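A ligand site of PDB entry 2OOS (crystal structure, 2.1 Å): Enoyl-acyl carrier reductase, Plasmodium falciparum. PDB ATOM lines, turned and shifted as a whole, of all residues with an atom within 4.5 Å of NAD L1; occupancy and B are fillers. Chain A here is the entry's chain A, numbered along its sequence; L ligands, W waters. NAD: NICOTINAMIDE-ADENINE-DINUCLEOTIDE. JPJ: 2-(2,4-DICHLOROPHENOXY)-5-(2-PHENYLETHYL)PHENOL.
An oxygen (O2N) of NAD L1 sits at hydrogen-bond distance from the side-chain hydroxyl (OG) of Ser 230, 2.7 Å away.
N of Tyr 24 lies within hydrogen-bond range of O1N of NAD L1 (2.7 Å).
N1A of NAD L1 is in hydrogen-bond range of N of Ala 82, 2.8 Å away.
An oxygen (O7N) of NAD L1 lies within hydrogen-bond range of the backbone NH (N) of Leu 228.
N7N of NAD L1 sits at hydrogen-bond distance from O of Leu 228.
The side-chain amino group (NZ) of Lys 198 lies within hydrogen-bond range of an oxygen (O2D) of NAD L1.
The backbone NH (N) of Ala 232 sits at hydrogen-bond distance from an oxygen (O1A) of NAD L1, at 3.1 Å.
OD1 of Asp 81 sits at hydrogen-bond distance from N6A of NAD L1, at 3.1 Å.
O3B of NAD L1 lies within hydrogen-bond range of N of Gly 19 (3.2 Å).
An oxygen (O3D) of NAD L1 is in hydrogen-bond range of the backbone carbonyl oxygen (O) of Leu 129 (3.2 Å).
OD1 of Asn 131 sits close to N7A of NAD L1, at 3.3 Å.
The side-chain hydroxyl (OH) of Tyr 190 lies within hydrogen-bond range of an oxygen (O22) of JPJ L2 (2.4 Å).
O2D of NAD L1 sits at hydrogen-bond distance from O22 of JPJ L2 (2.6 Å).
OG of Ser 230 lies within hydrogen-bond range of N of Ala 233.
The side-chain hydroxyl (OH) of Tyr 24 is in hydrogen-bond range of the backbone carbonyl oxygen (O) of Gly 226.
The backbone carbonyl oxygen (O) of Leu 178 sits at hydrogen-bond distance from the side-chain amino group (NZ) of Lys 198 (2.8 Å).
The backbone carbonyl oxygen (O) of Thr 179 is in hydrogen-bond range of the backbone NH (N) of Ala 225 (3.2 Å).
The side-chain carboxylate of Asp 81 is in hydrogen-bond range of the side-chain hydroxyl of Ser 83 (2.7 Å).
The side-chain hydroxyl (OG) of Ser 128 is in hydrogen-bond range of the backbone NH (N) of Gly 25.
NE of Arg 231 is in salt-bridge range of OD2 of Asp 20 (3.1 Å).
N6A of NAD L1 sits close to NE1 of Trp 44 (3.5 Å).
Residues that only touch NAD L1: Thr 179 (3.1 Å), Pro 227 (3.2 Å), Gly 23 (3.2 Å), Ser 128 (3.2 Å), Ala 225 (3.3 Å), Phe 80 (3.4 Å), Gly 226 (3.4 Å), Leu 178 (3.4 Å), Ile 18 (3.4 Å), Ala 130 (3.5 Å), Tyr 180 (3.7 Å), Arg 231 (3.8 Å), Gly 17 (3.8 Å) and Ser 83 (3.95 Å).
Hydrophobic or aromatic side chains that line NAD L1: Tyr 24, Trp 44, Ala 82, Leu 129, Ala 130, Leu 178, Tyr 180, Ala 225, Leu 228 and Ala 232.
25 residues have an atom within 4 Å of NAD L1: Gly 17, Ile 18, Gly 19, Gly 23, Tyr 24, Trp 44, Phe 80, Asp 81, Ala 82, Ser 83, Ser 128, Leu 129, Ala 130, Asn 131, Leu 178, Thr 179, Tyr 180, Lys 198, Ala 225, Gly 226, Pro 227, Leu 228, Ser 230, Arg 231 and Ala 232.
Water W5 lies within hydrogen-bond range of O of Ile 18 (2.5 Å), O2B of NAD L1 (2.8 Å) and N of Trp 44 (2.8 Å).
Water W1 lies within hydrogen-bond range of an oxygen (O3D) of NAD L1, the backbone carbonyl oxygen of Leu 178 and the backbone carbonyl oxygen of Leu 129.
Water W6 bridges the side-chain amino group (NZ) of Lys 153 and a nitrogen (N6A) of NAD L1.
Water W4 bridges O1A of NAD L1 (3.0 Å) and OD2 of Asp 20 (3.1 Å).
Water W3 lies within hydrogen-bond range of O of Gly 17 (2.6 Å), N of Gly 25 (2.9 Å), OG of Ser 128 (3.1 Å) and O1N of NAD L1 (3.2 Å).
Water W9 lies within hydrogen-bond range of NZ of Lys 198 (2.5 Å), O of Leu 129 (2.8 Å) and O3D of NAD L1 (3.5 Å).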
ATOM      1  N   GLY A  17       0.457   7.934   4.308  1.00  0.00           N
ATOM      2  CA  GLY A  17       1.085   8.176   2.999  1.00  0.00           C
ATOM      3  C   GLY A  17       0.586   9.409   2.254  1.00  0.00           C
ATOM      4  O   GLY A  17       0.174   9.343   1.098  1.00  0.00           O
ATOM      5  N   ILE A  18       0.615  10.536   2.906  1.00  0.00           N
ATOM      6  CA  ILE A  18       0.362  11.808   2.214  1.00  0.00           C
ATOM      7  C   ILE A  18       1.623  12.671   2.392  1.00  0.00           C
ATOM      8  O   ILE A  18       2.222  12.672   3.460  1.00  0.00           O
ATOM      9  CB  ILE A  18      -0.840  12.473   2.785  1.00  0.00           C
ATOM     10  CG1 ILE A  18      -1.216  13.715   1.989  1.00  0.00           C
ATOM     11  CG2 ILE A  18      -0.548  12.915   4.174  1.00  0.00           C
ATOM     12  CD1 ILE A  18      -1.909  14.705   2.855  1.00  0.00           C
ATOM     13  N   GLY A  19       2.056  13.354   1.324  1.00  0.00           N
ATOM     14  CA  GLY A  19       3.227  14.228   1.376  1.00  0.00           C
ATOM     15  C   GLY A  19       2.918  15.601   0.802  1.00  0.00           C
ATOM     16  O   GLY A  19       3.740  16.508   0.876  1.00  0.00           O
ATOM     17  N   ASP A  20       1.728  15.718   0.200  1.00  0.00           N
ATOM     18  CA  ASP A  20       1.285  16.872  -0.582  1.00  0.00           C
ATOM     19  C   ASP A  20      -0.148  16.579  -1.063  1.00  0.00           C
ATOM     20  O   ASP A  20      -0.737  15.543  -0.697  1.00  0.00           O
ATOM     21  CB  ASP A  20       2.240  17.169  -1.758  1.00  0.00           C
ATOM     22  CG  ASP A  20       2.355  15.982  -2.735  1.00  0.00           C
ATOM     23  OD1 ASP A  20       1.317  15.389  -3.113  1.00  0.00           O
ATOM     24  OD2 ASP A  20       3.479  15.680  -3.143  1.00  0.00           O
ATOM     25  N   GLY A  23      -1.256  13.328  -4.677  1.00  0.00           N
ATOM     26  CA  GLY A  23      -1.302  11.835  -4.684  1.00  0.00           C
ATOM     27  C   GLY A  23      -2.684  11.264  -4.452  1.00  0.00           C
ATOM     28  O   GLY A  23      -3.663  12.022  -4.309  1.00  0.00           O
ATOM     29  N   TYR A  24      -2.751   9.928  -4.382  1.00  0.00           N
ATOM     30  CA  TYR A  24      -3.995   9.247  -4.101  1.00  0.00           C
ATOM     31  C   TYR A  24      -4.487   9.472  -2.668  1.00  0.00           C
ATOM     32  O   TYR A  24      -5.683   9.464  -2.414  1.00  0.00           O
ATOM     33  CB  TYR A  24      -3.865   7.743  -4.433  1.00  0.00           C
ATOM     34  CG  TYR A  24      -4.034   7.521  -5.938  1.00  0.00           C
ATOM     35  CD1 TYR A  24      -5.160   8.015  -6.613  1.00  0.00           C
ATOM     36  CD2 TYR A  24      -3.068   6.854  -6.693  1.00  0.00           C
ATOM     37  CE1 TYR A  24      -5.326   7.843  -8.002  1.00  0.00           C
ATOM     38  CE2 TYR A  24      -3.229   6.672  -8.073  1.00  0.00           C
ATOM     39  CZ  TYR A  24      -4.350   7.164  -8.720  1.00  0.00           C
ATOM     40  OH  TYR A  24      -4.536   6.976 -10.066  1.00  0.00           O
ATOM     41  N   GLY A  25      -3.584   9.623  -1.721  1.00  0.00           N
ATOM     42  CA  GLY A  25      -4.035   9.735  -0.303  1.00  0.00           C
ATOM     43  C   GLY A  25      -4.955  10.959  -0.112  1.00  0.00           C
ATOM     44  O   GLY A  25      -5.989  10.879   0.586  1.00  0.00           O
ATOM     45  N   TRP A  44       5.270  10.890   6.202  1.00  0.00           N
ATOM     46  CA  TRP A  44       6.659  10.426   6.265  1.00  0.00           C
ATOM     47  C   TRP A  44       7.559  11.529   6.890  1.00  0.00           C
ATOM     48  O   TRP A  44       7.503  12.674   6.459  1.00  0.00           O
ATOM     49  CB  TRP A  44       7.087   9.998   4.867  1.00  0.00           C
ATOM     50  CG  TRP A  44       8.423   9.375   4.785  1.00  0.00           C
ATOM     51  CD1 TRP A  44       8.930   8.416   5.591  1.00  0.00           C
ATOM     52  CD2 TRP A  44       9.390   9.620   3.765  1.00  0.00           C
ATOM     53  NE1 TRP A  44      10.194   8.079   5.177  1.00  0.00           N
ATOM     54  CE2 TRP A  44      10.509   8.813   4.072  1.00  0.00           C
ATOM     55  CE3 TRP A  44       9.452  10.480   2.662  1.00  0.00           C
ATOM     56  CZ2 TRP A  44      11.676   8.802   3.283  1.00  0.00           C
ATOM     57  CZ3 TRP A  44      10.620  10.492   1.874  1.00  0.00           C
ATOM     58  CH2 TRP A  44      11.713   9.648   2.193  1.00  0.00           C
ATOM     59  N   VAL A  47       9.276  14.605   5.128  1.00  0.00           N
ATOM     60  CA  VAL A  47       8.489  15.660   4.509  1.00  0.00           C
ATOM     61  C   VAL A  47       7.427  16.231   5.456  1.00  0.00           C
ATOM     62  O   VAL A  47       6.567  16.979   5.020  1.00  0.00           O
ATOM     63  CB  VAL A  47       7.843  15.215   3.150  1.00  0.00           C
ATOM     64  CG1 VAL A  47       8.962  14.715   2.138  1.00  0.00           C
ATOM     65  CG2 VAL A  47       6.691  14.165   3.356  1.00  0.00           C
ATOM     66  N   PHE A  80       4.818   9.707  10.541  1.00  0.00           N
ATOM     67  CA  PHE A  80       4.592   8.266  10.457  1.00  0.00           C
ATOM     68  C   PHE A  80       5.620   7.685   9.474  1.00  0.00           C
ATOM     69  O   PHE A  80       5.692   8.122   8.326  1.00  0.00           O
ATOM     70  CB  PHE A  80       3.128   7.998  10.004  1.00  0.00           C
ATOM     71  CG  PHE A  80       2.849   6.549   9.664  1.00  0.00           C
ATOM     72  CD1 PHE A  80       2.452   5.637  10.668  1.00  0.00           C
ATOM     73  CD2 PHE A  80       3.013   6.086   8.349  1.00  0.00           C
ATOM     74  CE1 PHE A  80       2.196   4.285  10.352  1.00  0.00           C
ATOM     75  CE2 PHE A  80       2.775   4.720   8.029  1.00  0.00           C
ATOM     76  CZ  PHE A  80       2.377   3.831   9.024  1.00  0.00           C
ATOM     77  N   ASP A  81       6.421   6.724   9.955  1.00  0.00           N
ATOM     78  CA  ASP A  81       7.442   6.046   9.149  1.00  0.00           C
ATOM     79  C   ASP A  81       7.188   4.538   9.116  1.00  0.00           C
ATOM     80  O   ASP A  81       7.350   3.833  10.112  1.00  0.00           O
ATOM     81  CB  ASP A  81       8.853   6.331   9.685  1.00  0.00           C
ATOM     82  CG  ASP A  81       9.940   6.008   8.661  1.00  0.00           C
ATOM     83  OD1 ASP A  81       9.720   5.110   7.835  1.00  0.00           O
ATOM     84  OD2 ASP A  81      10.992   6.678   8.666  1.00  0.00           O
ATOM     85  N   ALA A  82       6.807   4.056   7.933  1.00  0.00           N
ATOM     86  CA  ALA A  82       6.397   2.675   7.692  1.00  0.00           C
ATOM     87  C   ALA A  82       7.564   1.690   7.712  1.00  0.00           C
ATOM     88  O   ALA A  82       7.375   0.468   7.619  1.00  0.00           O
ATOM     89  CB  ALA A  82       5.669   2.620   6.306  1.00  0.00           C
ATOM     90  N   SER A  83       8.787   2.193   7.798  1.00  0.00           N
ATOM     91  CA  SER A  83       9.898   1.286   7.935  1.00  0.00           C
ATOM     92  C   SER A  83      10.192   0.812   9.344  1.00  0.00           C
ATOM     93  O   SER A  83      10.978  -0.116   9.494  1.00  0.00           O
ATOM     94  CB  SER A  83      11.146   1.829   7.267  1.00  0.00           C
ATOM     95  OG  SER A  83      11.532   3.042   7.794  1.00  0.00           O
ATOM     96  N   SER A 128      -1.384   4.060   1.838  1.00  0.00           N
ATOM     97  CA  SER A 128      -1.269   4.762   0.550  1.00  0.00           C
ATOM     98  C   SER A 128       0.177   5.138   0.334  1.00  0.00           C
ATOM     99  O   SER A 128       0.486   6.300   0.097  1.00  0.00           O
ATOM    100  CB  SER A 128      -2.133   6.037   0.511  1.00  0.00           C
ATOM    101  OG  SER A 128      -2.136   6.579  -0.820  1.00  0.00           O
ATOM    102  N   LEU A 129       1.079   4.185   0.422  1.00  0.00           N
ATOM    103  CA  LEU A 129       2.492   4.516   0.462  1.00  0.00           C
ATOM    104  C   LEU A 129       3.297   3.408  -0.168  1.00  0.00           C
ATOM    105  O   LEU A 129       2.900   2.251  -0.160  1.00  0.00           O
ATOM    106  CB  LEU A 129       2.964   4.744   1.905  1.00  0.00           C
ATOM    107  CG  LEU A 129       2.928   3.562   2.867  1.00  0.00           C
ATOM    108  CD1 LEU A 129       4.305   2.885   2.896  1.00  0.00           C
ATOM    109  CD2 LEU A 129       2.525   4.011   4.273  1.00  0.00           C
ATOM    110  N   ALA A 130       4.451   3.796  -0.690  1.00  0.00           N
ATOM    111  CA  ALA A 130       5.412   2.880  -1.301  1.00  0.00           C
ATOM    112  C   ALA A 130       6.761   3.564  -1.284  1.00  0.00           C
ATOM    113  O   ALA A 130       6.831   4.793  -1.302  1.00  0.00           O
ATOM    114  CB  ALA A 130       5.025   2.570  -2.745  1.00  0.00           C
ATOM    115  N   ASN A 131       7.824   2.758  -1.222  1.00  0.00           N
ATOM    116  CA  ASN A 131       9.169   3.231  -1.505  1.00  0.00           C
ATOM    117  C   ASN A 131      10.013   2.038  -1.904  1.00  0.00           C
ATOM    118  O   ASN A 131       9.688   0.909  -1.580  1.00  0.00           O
ATOM    119  CB  ASN A 131       9.792   3.942  -0.274  1.00  0.00           C
ATOM    120  CG  ASN A 131      10.670   5.137  -0.656  1.00  0.00           C
ATOM    121  OD1 ASN A 131      10.787   6.080   0.150  1.00  0.00           O
ATOM    122  ND2 ASN A 131      11.262   5.136  -1.865  1.00  0.00           N
ATOM    123  N   LYS A 153       9.144  -1.547   2.787  1.00  0.00           N
ATOM    124  CA  LYS A 153       8.349  -0.313   2.856  1.00  0.00           C
ATOM    125  C   LYS A 153       6.989  -0.396   2.175  1.00  0.00           C
ATOM    126  O   LYS A 153       6.065   0.300   2.589  1.00  0.00           O
ATOM    127  CB  LYS A 153       9.078   0.872   2.234  1.00  0.00           C
ATOM    128  CG  LYS A 153      10.521   1.177   2.745  1.00  0.00           C
ATOM    129  CD  LYS A 153      10.727   0.980   4.261  1.00  0.00           C
ATOM    130  CE  LYS A 153      12.262   0.887   4.593  1.00  0.00           C
ATOM    131  NZ  LYS A 153      13.085   2.076   4.017  1.00  0.00           N
ATOM    132  N   LEU A 178      -3.190   0.615  -1.836  1.00  0.00           N
ATOM    133  CA  LEU A 178      -3.119   0.885  -3.272  1.00  0.00           C
ATOM    134  C   LEU A 178      -2.046   0.035  -3.968  1.00  0.00           C
ATOM    135  O   LEU A 178      -0.929  -0.100  -3.476  1.00  0.00           O
ATOM    136  CB  LEU A 178      -2.766   2.376  -3.480  1.00  0.00           C
ATOM    137  CG  LEU A 178      -3.838   3.481  -3.273  1.00  0.00           C
ATOM    138  CD1 LEU A 178      -5.022   3.296  -4.267  1.00  0.00           C
ATOM    139  CD2 LEU A 178      -4.371   3.451  -1.903  1.00  0.00           C
ATOM    140  N   THR A 179      -2.379  -0.509  -5.113  1.00  0.00           N
ATOM    141  CA  THR A 179      -1.479  -1.327  -5.818  1.00  0.00           C
ATOM    142  C   THR A 179      -1.438  -0.896  -7.307  1.00  0.00           C
ATOM    143  O   THR A 179      -2.064   0.069  -7.716  1.00  0.00           O
ATOM    144  CB  THR A 179      -1.831  -2.856  -5.653  1.00  0.00           C
ATOM    145  OG1 THR A 179      -0.756  -3.664  -6.183  1.00  0.00           O
ATOM    146  CG2 THR A 179      -3.132  -3.221  -6.416  1.00  0.00           C
ATOM    147  N   TYR A 180      -0.651  -1.619  -8.097  1.00  0.00           N
ATOM    148  CA  TYR A 180      -0.489  -1.322  -9.505  1.00  0.00           C
ATOM    149  C   TYR A 180      -0.308  -2.634 -10.269  1.00  0.00           C
ATOM    150  O   TYR A 180       0.286  -3.581  -9.782  1.00  0.00           O
ATOM    151  CB  TYR A 180       0.692  -0.334  -9.721  1.00  0.00           C
ATOM    152  CG  TYR A 180       0.890   0.079 -11.197  1.00  0.00           C
ATOM    153  CD1 TYR A 180      -0.139   0.704 -11.920  1.00  0.00           C
ATOM    154  CD2 TYR A 180       2.120  -0.159 -11.842  1.00  0.00           C
ATOM    155  CE1 TYR A 180       0.021   1.039 -13.295  1.00  0.00           C
ATOM    156  CE2 TYR A 180       2.320   0.214 -13.190  1.00  0.00           C
ATOM    157  CZ  TYR A 180       1.247   0.795 -13.909  1.00  0.00           C
ATOM    158  OH  TYR A 180       1.431   1.120 -15.217  1.00  0.00           O
ATOM    159  N   TYR A 190       9.187  -0.129 -14.139  1.00  0.00           N
ATOM    160  CA  TYR A 190       8.671  -0.194 -12.775  1.00  0.00           C
ATOM    161  C   TYR A 190       9.633  -1.089 -12.021  1.00  0.00           C
ATOM    162  O   TYR A 190       9.351  -2.268 -11.810  1.00  0.00           O
ATOM    163  CB  TYR A 190       7.263  -0.752 -12.772  1.00  0.00           C
ATOM    164  CG  TYR A 190       6.439  -0.474 -11.532  1.00  0.00           C
ATOM    165  CD1 TYR A 190       6.029   0.821 -11.199  1.00  0.00           C
ATOM    166  CD2 TYR A 190       6.010  -1.536 -10.728  1.00  0.00           C
ATOM    167  CE1 TYR A 190       5.246   1.057 -10.061  1.00  0.00           C
ATOM    168  CE2 TYR A 190       5.228  -1.308  -9.611  1.00  0.00           C
ATOM    169  CZ  TYR A 190       4.836  -0.027  -9.282  1.00  0.00           C
ATOM    170  OH  TYR A 190       4.050   0.143  -8.159  1.00  0.00           O
ATOM    171  N   LYS A 198       4.319  -5.183  -5.108  1.00  0.00           N
ATOM    172  CA  LYS A 198       2.885  -5.052  -5.384  1.00  0.00           C
ATOM    173  C   LYS A 198       2.242  -6.451  -5.495  1.00  0.00           C
ATOM    174  O   LYS A 198       1.100  -6.645  -5.102  1.00  0.00           O
ATOM    175  CB  LYS A 198       2.616  -4.236  -6.699  1.00  0.00           C
ATOM    176  CG  LYS A 198       2.975  -2.753  -6.553  1.00  0.00           C
ATOM    177  CD  LYS A 198       2.428  -2.086  -5.259  1.00  0.00           C
ATOM    178  CE  LYS A 198       2.339  -0.491  -5.384  1.00  0.00           C
ATOM    179  NZ  LYS A 198       1.839   0.053  -4.016  1.00  0.00           N
ATOM    180  N   ALA A 225      -4.810   1.082  -9.063  1.00  0.00           N
ATOM    181  CA  ALA A 225      -5.038   2.374  -9.666  1.00  0.00           C
ATOM    182  C   ALA A 225      -4.305   2.557 -10.987  1.00  0.00           C
ATOM    183  O   ALA A 225      -3.222   1.997 -11.225  1.00  0.00           O
ATOM    184  CB  ALA A 225      -4.634   3.467  -8.673  1.00  0.00           C
ATOM    185  N   GLY A 226      -4.903   3.310 -11.885  1.00  0.00           N
ATOM    186  CA  GLY A 226      -4.239   3.711 -13.096  1.00  0.00           C
ATOM    187  C   GLY A 226      -3.311   4.869 -12.737  1.00  0.00           C
ATOM    188  O   GLY A 226      -3.205   5.246 -11.555  1.00  0.00           O
ATOM    189  N   PRO A 227      -2.638   5.443 -13.752  1.00  0.00           N
ATOM    190  CA  PRO A 227      -1.538   6.377 -13.511  1.00  0.00           C
ATOM    191  C   PRO A 227      -2.037   7.778 -13.124  1.00  0.00           C
ATOM    192  O   PRO A 227      -3.064   8.249 -13.645  1.00  0.00           O
ATOM    193  CB  PRO A 227      -0.795   6.421 -14.844  1.00  0.00           C
ATOM    194  CG  PRO A 227      -1.848   6.093 -15.891  1.00  0.00           C
ATOM    195  CD  PRO A 227      -2.900   5.223 -15.190  1.00  0.00           C
ATOM    196  N   LEU A 228      -1.332   8.381 -12.169  1.00  0.00           N
ATOM    197  CA  LEU A 228      -1.615   9.719 -11.661  1.00  0.00           C
ATOM    198  C   LEU A 228      -0.247  10.408 -11.484  1.00  0.00           C
ATOM    199  O   LEU A 228       0.711   9.804 -10.961  1.00  0.00           O
ATOM    200  CB  LEU A 228      -2.315   9.620 -10.279  1.00  0.00           C
ATOM    201  CG  LEU A 228      -2.657  10.899  -9.500  1.00  0.00           C
ATOM    202  CD1 LEU A 228      -3.776  11.625 -10.282  1.00  0.00           C
ATOM    203  CD2 LEU A 228      -3.073  10.631  -8.037  1.00  0.00           C
ATOM    204  N   SER A 230       1.679  11.963  -9.473  1.00  0.00           N
ATOM    205  CA  SER A 230       1.994  12.203  -8.074  1.00  0.00           C
ATOM    206  C   SER A 230       3.488  12.458  -7.952  1.00  0.00           C
ATOM    207  O   SER A 230       4.259  12.201  -8.916  1.00  0.00           O
ATOM    208  CB  SER A 230       1.630  10.960  -7.274  1.00  0.00           C
ATOM    209  OG  SER A 230       2.538   9.930  -7.600  1.00  0.00           O
ATOM    210  N   ARG A 231       3.909  12.964  -6.794  1.00  0.00           N
ATOM    211  CA  ARG A 231       5.338  13.180  -6.542  1.00  0.00           C
ATOM    212  C   ARG A 231       6.153  11.912  -6.758  1.00  0.00           C
ATOM    213  O   ARG A 231       7.226  11.954  -7.385  1.00  0.00           O
ATOM    214  CB  ARG A 231       5.606  13.683  -5.114  1.00  0.00           C
ATOM    215  CG  ARG A 231       7.121  14.028  -4.927  1.00  0.00           C
ATOM    216  CD  ARG A 231       7.440  14.687  -3.557  1.00  0.00           C
ATOM    217  NE  ARG A 231       6.577  15.843  -3.270  1.00  0.00           N
ATOM    218  CZ  ARG A 231       6.656  16.637  -2.194  1.00  0.00           C
ATOM    219  NH1 ARG A 231       7.605  16.434  -1.272  1.00  0.00           N
ATOM    220  NH2 ARG A 231       5.797  17.653  -2.061  1.00  0.00           N
ATOM    221  N   ALA A 232       5.675  10.789  -6.215  1.00  0.00           N
ATOM    222  CA  ALA A 232       6.392   9.538  -6.342  1.00  0.00           C
ATOM    223  C   ALA A 232       6.530   9.117  -7.792  1.00  0.00           C
ATOM    224  O   ALA A 232       7.598   8.655  -8.203  1.00  0.00           O
ATOM    225  CB  ALA A 232       5.735   8.406  -5.494  1.00  0.00           C
ATOM    226  N   ALA A 233       5.455   9.294  -8.572  1.00  0.00           N
ATOM    227  CA  ALA A 233       5.427   8.901  -9.982  1.00  0.00           C
ATOM    228  C   ALA A 233       6.471   9.663 -10.802  1.00  0.00           C
ATOM    229  O   ALA A 233       7.142   9.071 -11.643  1.00  0.00           O
ATOM    230  CB  ALA A 233       4.056   9.113 -10.587  1.00  0.00           C
ATOM    231  N   ILE A 282       5.915   8.447 -16.285  1.00  0.00           N
ATOM    232  CA  ILE A 282       4.554   8.780 -15.855  1.00  0.00           C
ATOM    233  C   ILE A 282       3.767   9.557 -16.902  1.00  0.00           C
ATOM    234  O   ILE A 282       2.598   9.271 -17.142  1.00  0.00           O
ATOM    235  CB  ILE A 282       4.461   9.471 -14.432  1.00  0.00           C
ATOM    236  CG1 ILE A 282       2.998   9.623 -13.999  1.00  0.00           C
ATOM    237  CG2 ILE A 282       5.206  10.827 -14.382  1.00  0.00           C
ATOM    238  CD1 ILE A 282       2.294   8.270 -13.730  1.00  0.00           C
HETATM  239  PA  NAD L   1       2.645  10.059  -3.346  1.00  0.00           P
HETATM  240  O1A NAD L   1       4.047  10.549  -3.647  1.00  0.00           O
HETATM  241  O2A NAD L   1       1.501  11.033  -3.228  1.00  0.00           O
HETATM  242  O5B NAD L   1       2.515   9.167  -2.030  1.00  0.00           O
HETATM  243  C5B NAD L   1       3.478   8.195  -1.638  1.00  0.00           C
HETATM  244  C4B NAD L   1       3.705   8.472  -0.170  1.00  0.00           C
HETATM  245  O4B NAD L   1       4.468   7.454   0.486  1.00  0.00           O
HETATM  246  C3B NAD L   1       4.528   9.754  -0.057  1.00  0.00           C
HETATM  247  O3B NAD L   1       3.711  10.746   0.565  1.00  0.00           O
HETATM  248  C2B NAD L   1       5.715   9.399   0.832  1.00  0.00           C
HETATM  249  O2B NAD L   1       5.988  10.487   1.745  1.00  0.00           O
HETATM  250  C1B NAD L   1       5.243   8.114   1.505  1.00  0.00           C
HETATM  251  N9A NAD L   1       6.360   7.281   2.043  1.00  0.00           N
HETATM  252  C8A NAD L   1       7.506   6.915   1.393  1.00  0.00           C
HETATM  253  N7A NAD L   1       8.281   6.205   2.254  1.00  0.00           N
HETATM  254  C5A NAD L   1       7.604   6.095   3.429  1.00  0.00           C
HETATM  255  C6A NAD L   1       7.901   5.473   4.652  1.00  0.00           C
HETATM  256  N6A NAD L   1       9.067   4.786   4.828  1.00  0.00           N
HETATM  257  N1A NAD L   1       7.026   5.586   5.654  1.00  0.00           N
HETATM  258  C2A NAD L   1       5.859   6.288   5.521  1.00  0.00           C
HETATM  259  N3A NAD L   1       5.530   6.898   4.352  1.00  0.00           N
HETATM  260  C4A NAD L   1       6.393   6.797   3.303  1.00  0.00           C
HETATM  261  O3  NAD L   1       2.360   9.048  -4.576  1.00  0.00           O
HETATM  262  PN  NAD L   1       1.052   8.213  -4.927  1.00  0.00           P
HETATM  263  O1N NAD L   1      -0.224   8.867  -4.446  1.00  0.00           O
HETATM  264  O2N NAD L   1       1.260   7.871  -6.393  1.00  0.00           O
HETATM  265  O5D NAD L   1       1.276   6.865  -4.053  1.00  0.00           O
HETATM  266  C5D NAD L   1       0.369   6.270  -3.110  1.00  0.00           C
HETATM  267  C4D NAD L   1       0.142   4.787  -3.431  1.00  0.00           C
HETATM  268  O4D NAD L   1      -0.530   4.583  -4.696  1.00  0.00           O
HETATM  269  C3D NAD L   1       1.427   3.995  -3.508  1.00  0.00           C
HETATM  270  O3D NAD L   1       1.174   2.738  -2.860  1.00  0.00           O
HETATM  271  C2D NAD L   1       1.620   3.772  -4.992  1.00  0.00           C
HETATM  272  O2D NAD L   1       2.343   2.581  -5.197  1.00  0.00           O
HETATM  273  C1D NAD L   1       0.186   3.637  -5.491  1.00  0.00           C
HETATM  274  N1N NAD L   1      -0.091   3.813  -6.936  1.00  0.00           N
HETATM  275  C2N NAD L   1       0.194   4.983  -7.576  1.00  0.00           C
HETATM  276  C3N NAD L   1      -0.100   5.149  -8.937  1.00  0.00           C
HETATM  277  C7N NAD L   1       0.233   6.454  -9.655  1.00  0.00           C
HETATM  278  O7N NAD L   1       0.166   6.453 -10.844  1.00  0.00           O
HETATM  279  N7N NAD L   1       0.572   7.568  -8.995  1.00  0.00           N
HETATM  280  C4N NAD L   1      -0.699   4.098  -9.639  1.00  0.00           C
HETATM  281  C5N NAD L   1      -0.976   2.924  -8.951  1.00  0.00           C
HETATM  282  C6N NAD L   1      -0.672   2.807  -7.587  1.00  0.00           C
HETATM  283 CL20 JPJ L   2       4.542   5.858  -4.177  1.00  0.00          CL
HETATM  284  C15 JPJ L   2       5.662   5.067  -5.324  1.00  0.00           C
HETATM  285  C16 JPJ L   2       6.978   4.841  -4.935  1.00  0.00           C
HETATM  286  C17 JPJ L   2       7.867   4.226  -5.825  1.00  0.00           C
HETATM  287 CL21 JPJ L   2       9.527   3.987  -5.251  1.00  0.00          CL
HETATM  288  C22 JPJ L   2       7.471   3.863  -7.108  1.00  0.00           C
HETATM  289  C19 JPJ L   2       6.151   4.099  -7.497  1.00  0.00           C
HETATM  290  C14 JPJ L   2       5.250   4.695  -6.595  1.00  0.00           C
HETATM  291  O13 JPJ L   2       3.954   4.959  -6.945  1.00  0.00           O
HETATM  292  C2  JPJ L   2       3.537   4.686  -8.228  1.00  0.00           C
HETATM  293  C1  JPJ L   2       3.139   3.385  -8.586  1.00  0.00           C
HETATM  294  O22 JPJ L   2       3.214   2.382  -7.650  1.00  0.00           O
HETATM  295  C3  JPJ L   2       3.502   5.713  -9.190  1.00  0.00           C
HETATM  296  C4  JPJ L   2       3.073   5.438 -10.491  1.00  0.00           C
HETATM  297  C5  JPJ L   2       2.689   4.148 -10.872  1.00  0.00           C
HETATM  298  C6  JPJ L   2       2.697   3.130  -9.905  1.00  0.00           C
HETATM  299  C7  JPJ L   2       2.181   3.842 -12.285  1.00  0.00           C
HETATM  300  C18 JPJ L   2       2.781   4.617 -13.445  1.00  0.00           C
HETATM  301  C28 JPJ L   2       4.242   4.275 -13.659  1.00  0.00           C
HETATM  302  C27 JPJ L   2       4.611   3.112 -14.321  1.00  0.00           C
HETATM  303  C26 JPJ L   2       5.951   2.768 -14.524  1.00  0.00           C
HETATM  304  C25 JPJ L   2       6.939   3.624 -14.056  1.00  0.00           C
HETATM  305  C24 JPJ L   2       6.568   4.818 -13.392  1.00  0.00           C
HETATM  306  C23 JPJ L   2       5.226   5.141 -13.190  1.00  0.00           C
HETATM  307  O   HOH W   1      -0.332   1.286  -0.794  1.00  0.00           O
HETATM  308  O   HOH W   2       7.361   7.461  -2.019  1.00  0.00           O
HETATM  309  O   HOH W   3      -0.700   9.290  -1.311  1.00  0.00           O
HETATM  310  O   HOH W   4       4.262  12.964  -1.910  1.00  0.00           O
HETATM  311  O   HOH W   5       4.037  11.004   3.653  1.00  0.00           O
HETATM  312  O   HOH W   6      11.594   4.260   3.351  1.00  0.00           O
HETATM  313  O   HOH W   7       1.916  13.405  -4.813  1.00  0.00           O
HETATM  314  O   HOH W   8       0.798  12.621  -1.236  1.00  0.00           O
HETATM  315  O   HOH W   9       2.613  -0.173  -1.622  1.00  0.00           O
